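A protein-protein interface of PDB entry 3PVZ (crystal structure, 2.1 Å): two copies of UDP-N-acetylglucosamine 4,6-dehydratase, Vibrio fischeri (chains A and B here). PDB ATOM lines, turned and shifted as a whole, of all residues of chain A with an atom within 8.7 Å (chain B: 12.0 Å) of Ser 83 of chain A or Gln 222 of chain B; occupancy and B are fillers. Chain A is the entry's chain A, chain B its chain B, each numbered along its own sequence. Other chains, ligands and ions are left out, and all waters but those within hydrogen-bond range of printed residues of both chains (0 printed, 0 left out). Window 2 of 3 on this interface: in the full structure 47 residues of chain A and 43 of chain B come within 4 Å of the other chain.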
ATOM      1  N   LYS A  53      24.867  10.830  10.224  1.00  0.00           N
ATOM      2  CA  LYS A  53      24.440  12.176  10.621  1.00  0.00           C
ATOM      3  C   LYS A  53      25.134  12.570  11.929  1.00  0.00           C
ATOM      4  O   LYS A  53      25.692  13.644  12.001  1.00  0.00           O
ATOM      5  CB  LYS A  53      22.959  12.233  10.764  1.00  0.00           C
ATOM      6  CG  LYS A  53      22.293  12.004   9.424  1.00  0.00           C
ATOM      7  CD  LYS A  53      20.905  12.514   9.380  1.00  0.00           C
ATOM      8  CE  LYS A  53      19.984  11.646  10.164  1.00  0.00           C
ATOM      9  NZ  LYS A  53      18.570  12.169  10.031  1.00  0.00           N
ATOM     10  N   PHE A  56      28.522  13.588  10.731  1.00  0.00           N
ATOM     11  CA  PHE A  56      28.513  14.740   9.858  1.00  0.00           C
ATOM     12  C   PHE A  56      28.323  16.083  10.603  1.00  0.00           C
ATOM     13  O   PHE A  56      28.976  17.068  10.281  1.00  0.00           O
ATOM     14  CB  PHE A  56      27.415  14.575   8.806  1.00  0.00           C
ATOM     15  CG  PHE A  56      27.503  15.578   7.701  1.00  0.00           C
ATOM     16  CD1 PHE A  56      26.961  16.821   7.856  1.00  0.00           C
ATOM     17  CD2 PHE A  56      28.171  15.291   6.529  1.00  0.00           C
ATOM     18  CE1 PHE A  56      27.063  17.763   6.858  1.00  0.00           C
ATOM     19  CE2 PHE A  56      28.256  16.243   5.495  1.00  0.00           C
ATOM     20  CZ  PHE A  56      27.685  17.486   5.688  1.00  0.00           C
ATOM     21  N   LYS A  57      27.418  16.125  11.568  1.00  0.00           N
ATOM     22  CA  LYS A  57      27.076  17.368  12.263  1.00  0.00           C
ATOM     23  C   LYS A  57      28.219  17.831  13.168  1.00  0.00           C
ATOM     24  O   LYS A  57      28.210  18.971  13.641  1.00  0.00           O
ATOM     25  CB  LYS A  57      25.780  17.171  13.084  1.00  0.00           C
ATOM     26  CG  LYS A  57      25.861  16.220  14.260  1.00  0.00           C
ATOM     27  CD  LYS A  57      24.634  16.293  15.215  1.00  0.00           C
ATOM     28  CE  LYS A  57      23.508  15.362  14.804  1.00  0.00           C
ATOM     29  NZ  LYS A  57      22.420  15.192  15.896  1.00  0.00           N
ATOM     30  N   GLU A  75      18.408   9.792  -0.456  1.00  0.00           N
ATOM     31  CA  GLU A  75      17.702  10.294   0.701  1.00  0.00           C
ATOM     32  C   GLU A  75      18.624  10.766   1.871  1.00  0.00           C
ATOM     33  O   GLU A  75      18.378  11.809   2.511  1.00  0.00           O
ATOM     34  CB  GLU A  75      16.702   9.214   1.166  1.00  0.00           C
ATOM     35  CG  GLU A  75      16.014   9.488   2.445  1.00  0.00           C
ATOM     36  CD  GLU A  75      15.188  10.779   2.430  1.00  0.00           C
ATOM     37  OE1 GLU A  75      14.989  11.360   1.333  1.00  0.00           O
ATOM     38  OE2 GLU A  75      14.746  11.200   3.532  1.00  0.00           O
ATOM     39  N   LEU A  76      19.696  10.031   2.135  1.00  0.00           N
ATOM     40  CA  LEU A  76      20.616  10.398   3.199  1.00  0.00           C
ATOM     41  C   LEU A  76      21.253  11.742   2.904  1.00  0.00           C
ATOM     42  O   LEU A  76      21.371  12.613   3.786  1.00  0.00           O
ATOM     43  CB  LEU A  76      21.728   9.323   3.307  1.00  0.00           C
ATOM     44  CG  LEU A  76      22.902   9.698   4.206  1.00  0.00           C
ATOM     45  CD1 LEU A  76      22.398  10.016   5.597  1.00  0.00           C
ATOM     46  CD2 LEU A  76      24.017   8.603   4.251  1.00  0.00           C
ATOM     47  N   VAL A  77      21.729  11.899   1.687  1.00  0.00           N
ATOM     48  CA  VAL A  77      22.331  13.186   1.293  1.00  0.00           C
ATOM     49  C   VAL A  77      21.300  14.354   1.352  1.00  0.00           C
ATOM     50  O   VAL A  77      21.602  15.392   1.915  1.00  0.00           O
ATOM     51  CB  VAL A  77      22.937  13.107  -0.090  1.00  0.00           C
ATOM     52  CG1 VAL A  77      23.662  14.401  -0.442  1.00  0.00           C
ATOM     53  CG2 VAL A  77      23.884  11.925  -0.188  1.00  0.00           C
ATOM     54  N   ARG A  78      20.085  14.172   0.828  1.00  0.00           N
ATOM     55  CA  ARG A  78      19.068  15.237   0.899  1.00  0.00           C
ATOM     56  C   ARG A  78      18.754  15.631   2.345  1.00  0.00           C
ATOM     57  O   ARG A  78      18.720  16.785   2.668  1.00  0.00           O
ATOM     58  CB  ARG A  78      17.813  14.849   0.113  1.00  0.00           C
ATOM     59  CG  ARG A  78      18.102  14.784  -1.400  1.00  0.00           C
ATOM     60  CD  ARG A  78      16.850  14.612  -2.315  1.00  0.00           C
ATOM     61  NE  ARG A  78      17.257  14.237  -3.680  1.00  0.00           N
ATOM     62  CZ  ARG A  78      17.805  15.061  -4.585  1.00  0.00           C
ATOM     63  NH1 ARG A  78      18.000  16.356  -4.328  1.00  0.00           N
ATOM     64  NH2 ARG A  78      18.141  14.587  -5.781  1.00  0.00           N
ATOM     65  N   ASP A  79      18.554  14.668   3.209  1.00  0.00           N
ATOM     66  CA  ASP A  79      18.392  14.908   4.629  1.00  0.00           C
ATOM     67  C   ASP A  79      19.605  15.668   5.247  1.00  0.00           C
ATOM     68  O   ASP A  79      19.462  16.602   6.055  1.00  0.00           O
ATOM     69  CB  ASP A  79      18.268  13.520   5.275  1.00  0.00           C
ATOM     70  CG  ASP A  79      17.750  13.556   6.672  1.00  0.00           C
ATOM     71  OD1 ASP A  79      17.480  14.665   7.208  1.00  0.00           O
ATOM     72  OD2 ASP A  79      17.614  12.451   7.245  1.00  0.00           O
ATOM     73  N   ILE A  80      20.810  15.241   4.906  1.00  0.00           N
ATOM     74  CA  ILE A  80      21.998  15.900   5.431  1.00  0.00           C
ATOM     75  C   ILE A  80      22.053  17.339   4.907  1.00  0.00           C
ATOM     76  O   ILE A  80      22.371  18.252   5.651  1.00  0.00           O
ATOM     77  CB  ILE A  80      23.289  15.167   5.039  1.00  0.00           C
ATOM     78  CG1 ILE A  80      23.500  13.990   5.990  1.00  0.00           C
ATOM     79  CG2 ILE A  80      24.496  16.121   5.084  1.00  0.00           C
ATOM     80  CD1 ILE A  80      24.542  13.018   5.536  1.00  0.00           C
ATOM     81  N   ARG A  81      21.752  17.536   3.631  1.00  0.00           N
ATOM     82  CA  ARG A  81      21.806  18.886   3.067  1.00  0.00           C
ATOM     83  C   ARG A  81      20.835  19.815   3.776  1.00  0.00           C
ATOM     84  O   ARG A  81      21.194  20.928   4.110  1.00  0.00           O
ATOM     85  CB  ARG A  81      21.551  18.917   1.555  1.00  0.00           C
ATOM     86  CG  ARG A  81      22.500  18.005   0.714  1.00  0.00           C
ATOM     87  CD  ARG A  81      23.866  18.586   0.291  1.00  0.00           C
ATOM     88  NE  ARG A  81      24.868  18.584   1.362  1.00  0.00           N
ATOM     89  CZ  ARG A  81      26.068  17.987   1.336  1.00  0.00           C
ATOM     90  NH1 ARG A  81      26.863  18.101   2.401  1.00  0.00           N
ATOM     91  NH2 ARG A  81      26.502  17.305   0.275  1.00  0.00           N
ATOM     92  N   SER A  82      19.624  19.363   4.047  1.00  0.00           N
ATOM     93  CA  SER A  82      18.656  20.272   4.650  1.00  0.00           C
ATOM     94  C   SER A  82      18.823  20.408   6.164  1.00  0.00           C
ATOM     95  O   SER A  82      18.580  21.461   6.719  1.00  0.00           O
ATOM     96  CB  SER A  82      17.222  19.904   4.261  1.00  0.00           C
ATOM     97  OG  SER A  82      16.935  18.541   4.490  1.00  0.00           O
ATOM     98  N   SER A  83      19.274  19.361   6.828  1.00  0.00           N
ATOM     99  CA  SER A  83      19.557  19.453   8.252  1.00  0.00           C
ATOM    100  C   SER A  83      20.822  20.245   8.565  1.00  0.00           C
ATOM    101  O   SER A  83      20.804  21.056   9.476  1.00  0.00           O
ATOM    102  CB  SER A  83      19.689  18.069   8.875  1.00  0.00           C
ATOM    103  OG  SER A  83      18.454  17.387   8.804  1.00  0.00           O
ATOM    104  N   PHE A  84      21.922  19.982   7.843  1.00  0.00           N
ATOM    105  CA  PHE A  84      23.242  20.461   8.277  1.00  0.00           C
ATOM    106  C   PHE A  84      23.966  21.282   7.265  1.00  0.00           C
ATOM    107  O   PHE A  84      24.837  22.064   7.614  1.00  0.00           O
ATOM    108  CB  PHE A  84      24.119  19.282   8.684  1.00  0.00           C
ATOM    109  CG  PHE A  84      23.435  18.297   9.604  1.00  0.00           C
ATOM    110  CD1 PHE A  84      22.793  18.728  10.749  1.00  0.00           C
ATOM    111  CD2 PHE A  84      23.502  16.925   9.345  1.00  0.00           C
ATOM    112  CE1 PHE A  84      22.172  17.816  11.612  1.00  0.00           C
ATOM    113  CE2 PHE A  84      22.888  15.988  10.199  1.00  0.00           C
ATOM    114  CZ  PHE A  84      22.226  16.417  11.316  1.00  0.00           C
ATOM    115  N   GLY A  85      23.647  21.109   5.998  1.00  0.00           N
ATOM    116  CA  GLY A  85      24.329  21.865   4.954  1.00  0.00           C
ATOM    117  C   GLY A  85      25.610  21.136   4.519  1.00  0.00           C
ATOM    118  O   GLY A  85      25.564  19.963   4.184  1.00  0.00           O
ATOM    119  N   TYR A  86      26.723  21.861   4.498  1.00  0.00           N
ATOM    120  CA  TYR A  86      27.968  21.407   3.894  1.00  0.00           C
ATOM    121  C   TYR A  86      29.109  21.584   4.867  1.00  0.00           C
ATOM    122  O   TYR A  86      29.013  22.377   5.790  1.00  0.00           O
ATOM    123  CB  TYR A  86      28.280  22.178   2.601  1.00  0.00           C
ATOM    124  CG  TYR A  86      27.154  22.111   1.583  1.00  0.00           C
ATOM    125  CD1 TYR A  86      27.170  21.168   0.575  1.00  0.00           C
ATOM    126  CD2 TYR A  86      26.057  22.967   1.663  1.00  0.00           C
ATOM    127  CE1 TYR A  86      26.135  21.080  -0.353  1.00  0.00           C
ATOM    128  CE2 TYR A  86      25.015  22.898   0.731  1.00  0.00           C
ATOM    129  CZ  TYR A  86      25.070  21.952  -0.273  1.00  0.00           C
ATOM    130  OH  TYR A  86      24.059  21.840  -1.197  1.00  0.00           O
ATOM    131  N   ARG B 217      10.475  13.795   3.334  1.00  0.00           N
ATOM    132  CA  ARG B 217      10.455  15.236   3.654  1.00  0.00           C
ATOM    133  C   ARG B 217       9.351  15.640   4.627  1.00  0.00           C
ATOM    134  O   ARG B 217       9.613  16.434   5.529  1.00  0.00           O
ATOM    135  CB  ARG B 217      10.359  16.112   2.389  1.00  0.00           C
ATOM    136  CG  ARG B 217      11.504  15.916   1.386  1.00  0.00           C
ATOM    137  CD  ARG B 217      12.841  16.552   1.836  1.00  0.00           C
ATOM    138  NE  ARG B 217      13.588  15.799   2.850  1.00  0.00           N
ATOM    139  CZ  ARG B 217      14.192  14.619   2.672  1.00  0.00           C
ATOM    140  NH1 ARG B 217      14.143  13.969   1.515  1.00  0.00           N
ATOM    141  NH2 ARG B 217      14.854  14.066   3.684  1.00  0.00           N
ATOM    142  N   ILE B 218       8.129  15.130   4.437  1.00  0.00           N
ATOM    143  CA  ILE B 218       7.016  15.409   5.373  1.00  0.00           C
ATOM    144  C   ILE B 218       7.162  14.592   6.659  1.00  0.00           C
ATOM    145  O   ILE B 218       6.869  15.094   7.758  1.00  0.00           O
ATOM    146  CB  ILE B 218       5.602  15.139   4.749  1.00  0.00           C
ATOM    147  CG1 ILE B 218       5.378  16.019   3.515  1.00  0.00           C
ATOM    148  CG2 ILE B 218       4.474  15.414   5.775  1.00  0.00           C
ATOM    149  CD1 ILE B 218       5.224  17.504   3.841  1.00  0.00           C
ATOM    150  N   GLN B 219       7.602  13.339   6.516  1.00  0.00           N
ATOM    151  CA  GLN B 219       7.947  12.507   7.669  1.00  0.00           C
ATOM    152  C   GLN B 219       8.945  13.239   8.563  1.00  0.00           C
ATOM    153  O   GLN B 219       8.743  13.343   9.777  1.00  0.00           O
ATOM    154  CB  GLN B 219       8.531  11.163   7.227  1.00  0.00           C
ATOM    155  CG  GLN B 219       7.481  10.079   6.981  1.00  0.00           C
ATOM    156  CD  GLN B 219       7.979   8.704   7.382  1.00  0.00           C
ATOM    157  OE1 GLN B 219       8.482   7.950   6.548  1.00  0.00           O
ATOM    158  NE2 GLN B 219       7.872   8.385   8.672  1.00  0.00           N
ATOM    159  N   LYS B 220       9.984  13.796   7.943  1.00  0.00           N
ATOM    160  CA  LYS B 220      11.048  14.489   8.670  1.00  0.00           C
ATOM    161  C   LYS B 220      10.867  16.027   8.762  1.00  0.00           C
ATOM    162  O   LYS B 220      11.850  16.742   8.930  1.00  0.00           O
ATOM    163  CB  LYS B 220      12.390  14.171   8.006  1.00  0.00           C
ATOM    164  CG  LYS B 220      12.596  12.704   7.641  1.00  0.00           C
ATOM    165  CD  LYS B 220      13.950  12.519   6.965  1.00  0.00           C
ATOM    166  CE  LYS B 220      14.389  11.059   6.902  1.00  0.00           C
ATOM    167  NZ  LYS B 220      13.750  10.326   5.785  1.00  0.00           N
ATOM    168  N   ASN B 221       9.630  16.524   8.675  1.00  0.00           N
ATOM    169  CA  ASN B 221       9.338  17.980   8.639  1.00  0.00           C
ATOM    170  C   ASN B 221      10.446  18.822   8.000  1.00  0.00           C
ATOM    171  O   ASN B 221      11.002  19.744   8.613  1.00  0.00           O
ATOM    172  CB  ASN B 221       8.968  18.526  10.028  1.00  0.00           C
ATOM    173  CG  ASN B 221       7.710  17.888  10.577  1.00  0.00           C
ATOM    174  OD1 ASN B 221       7.625  16.663  10.680  1.00  0.00           O
ATOM    175  ND2 ASN B 221       6.714  18.706  10.912  1.00  0.00           N
ATOM    176  N   GLN B 222      10.760  18.469   6.759  1.00  0.00           N
ATOM    177  CA  GLN B 222      11.695  19.223   5.942  1.00  0.00           C
ATOM    178  C   GLN B 222      10.918  19.877   4.797  1.00  0.00           C
ATOM    179  O   GLN B 222       9.917  19.319   4.335  1.00  0.00           O
ATOM    180  CB  GLN B 222      12.804  18.299   5.411  1.00  0.00           C
ATOM    181  CG  GLN B 222      13.953  18.105   6.414  1.00  0.00           C
ATOM    182  CD  GLN B 222      14.819  16.863   6.152  1.00  0.00           C
ATOM    183  OE1 GLN B 222      14.711  16.210   5.116  1.00  0.00           O
ATOM    184  NE2 GLN B 222      15.688  16.552   7.099  1.00  0.00           N
ATOM    185  N   PRO B 223      11.370  21.063   4.340  1.00  0.00           N
ATOM    186  CA  PRO B 223      10.776  21.716   3.159  1.00  0.00           C
ATOM    187  C   PRO B 223      10.730  20.815   1.912  1.00  0.00           C
ATOM    188  O   PRO B 223      11.503  19.854   1.808  1.00  0.00           O
ATOM    189  CB  PRO B 223      11.723  22.895   2.898  1.00  0.00           C
ATOM    190  CG  PRO B 223      12.375  23.175   4.212  1.00  0.00           C
ATOM    191  CD  PRO B 223      12.455  21.869   4.938  1.00  0.00           C
ATOM    192  N   ILE B 224       9.827  21.115   0.978  1.00  0.00           N
ATOM    193  CA  ILE B 224       9.952  20.572  -0.387  1.00  0.00           C
ATOM    194  C   ILE B 224      10.222  21.734  -1.340  1.00  0.00           C
ATOM    195  O   ILE B 224      10.047  22.904  -0.965  1.00  0.00           O
ATOM    196  CB  ILE B 224       8.694  19.796  -0.851  1.00  0.00           C
ATOM    197  CG1 ILE B 224       8.275  18.753   0.193  1.00  0.00           C
ATOM    198  CG2 ILE B 224       8.967  19.117  -2.202  1.00  0.00           C
ATOM    199  CD1 ILE B 224       7.047  17.939  -0.210  1.00  0.00           C
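The side-chain carboxylate (OD1) of Asp 79 of chain A sits at hydrogen-bond distance from the side-chain amide nitrogen (NE2) of Gln 222 of chain B (2.6 Å). The side-chain hydroxyl (OG) of Ser 83 of chain A is in hydrogen-bond range of the side-chain amide nitrogen (NE2) of Gln 222 of chain B, at 3.4 Å. The side-chain amino group (NZ) of Lys 220 of chain B is in salt-bridge range of the side-chain carboxylate (OE2) of Glu 75 of chain A (2.6 Å). OE1 of Glu 75 of chain A lies within salt-bridge range of NH1 of Arg 217 of chain B. OG of Ser 82 of chain A lies close to OE1 of Gln 222 of chain B.
OG of Ser 83 of chain A is in hydrogen-bond range of O of Asp 79 of chain A (3.0 Å). The side-chain hydroxyl of Ser 82 of chain A is in hydrogen-bond range of the backbone carbonyl oxygen of Arg 78 of chain A (3.1 Å). OE1 of Gln 222 of chain B sits at hydrogen-bond distance from NE of Arg 217 of chain B, at 2.6 Å. OD2 of Asp 79 of chain A is in salt-bridge range of NZ of Lys 53 of chain A, 3.0 Å away.
Among the printed residues, pairs that only touch across the chains: Asp 79 of chain A with Lys 220 of chain B (3.5 Å) and Asp 79 of chain A with Arg 217 of chain B (3.8 Å).
Of the printed residues of chain B, Glu 75 of chain A touches Arg 217 (2.7 Å) and Lys 220 (2.6 Å). Of chain B, only Arg 217, Lys 220 and Gln 222 come within 4 Å of Asp 79 of chain A. No residue of chain B comes within 4 Å of Ile 80 of chain A. Ser 82 of chain A touches just one residue of chain B: Gln 222 (3.2 Å). Ser 83 of chain A touches just one residue of chain B: Gln 222. No residue of chain B comes within 4 Å of Phe 84 of chain A. No residue of chain B comes within 4 Å of Gly 85 of chain A. Of the printed residues of chain A, Arg 217 of chain B touches Glu 75 (2.7 Å) and Asp 79 (3.8 Å). Of the printed residues of chain A, Lys 220 of chain B touches Glu 75 and Asp 79. Of chain A, only Asp 79 (2.6 Å), Ser 82 (3.2 Å) and Ser 83 (3.4 Å) come within 4 Å of Gln 222 of chain B. The nearest residue of chain B that does not touch Ser 83 of chain A is Lys 220 of chain B (6.6 Å). The nearest printed residue of chain A that does not touch Gln 222 of chain B is Arg 78 of chain A (4.7 Å). The nearest printed residue of chain B that does not touch Glu 75 of chain A is Gln 222 of chain B (5.3 Å).
Among the printed residues, 7 pairs touch across the chains. Among the printed residues, Asp or Glu carboxylates within 4 Å of a Lys or Arg side-chain nitrogen of the other chain: Glu 75 of chain A with Arg 217 of chain B and Glu 75 of chain A with Lys 220 of chain B.
No position is printed for both chains.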
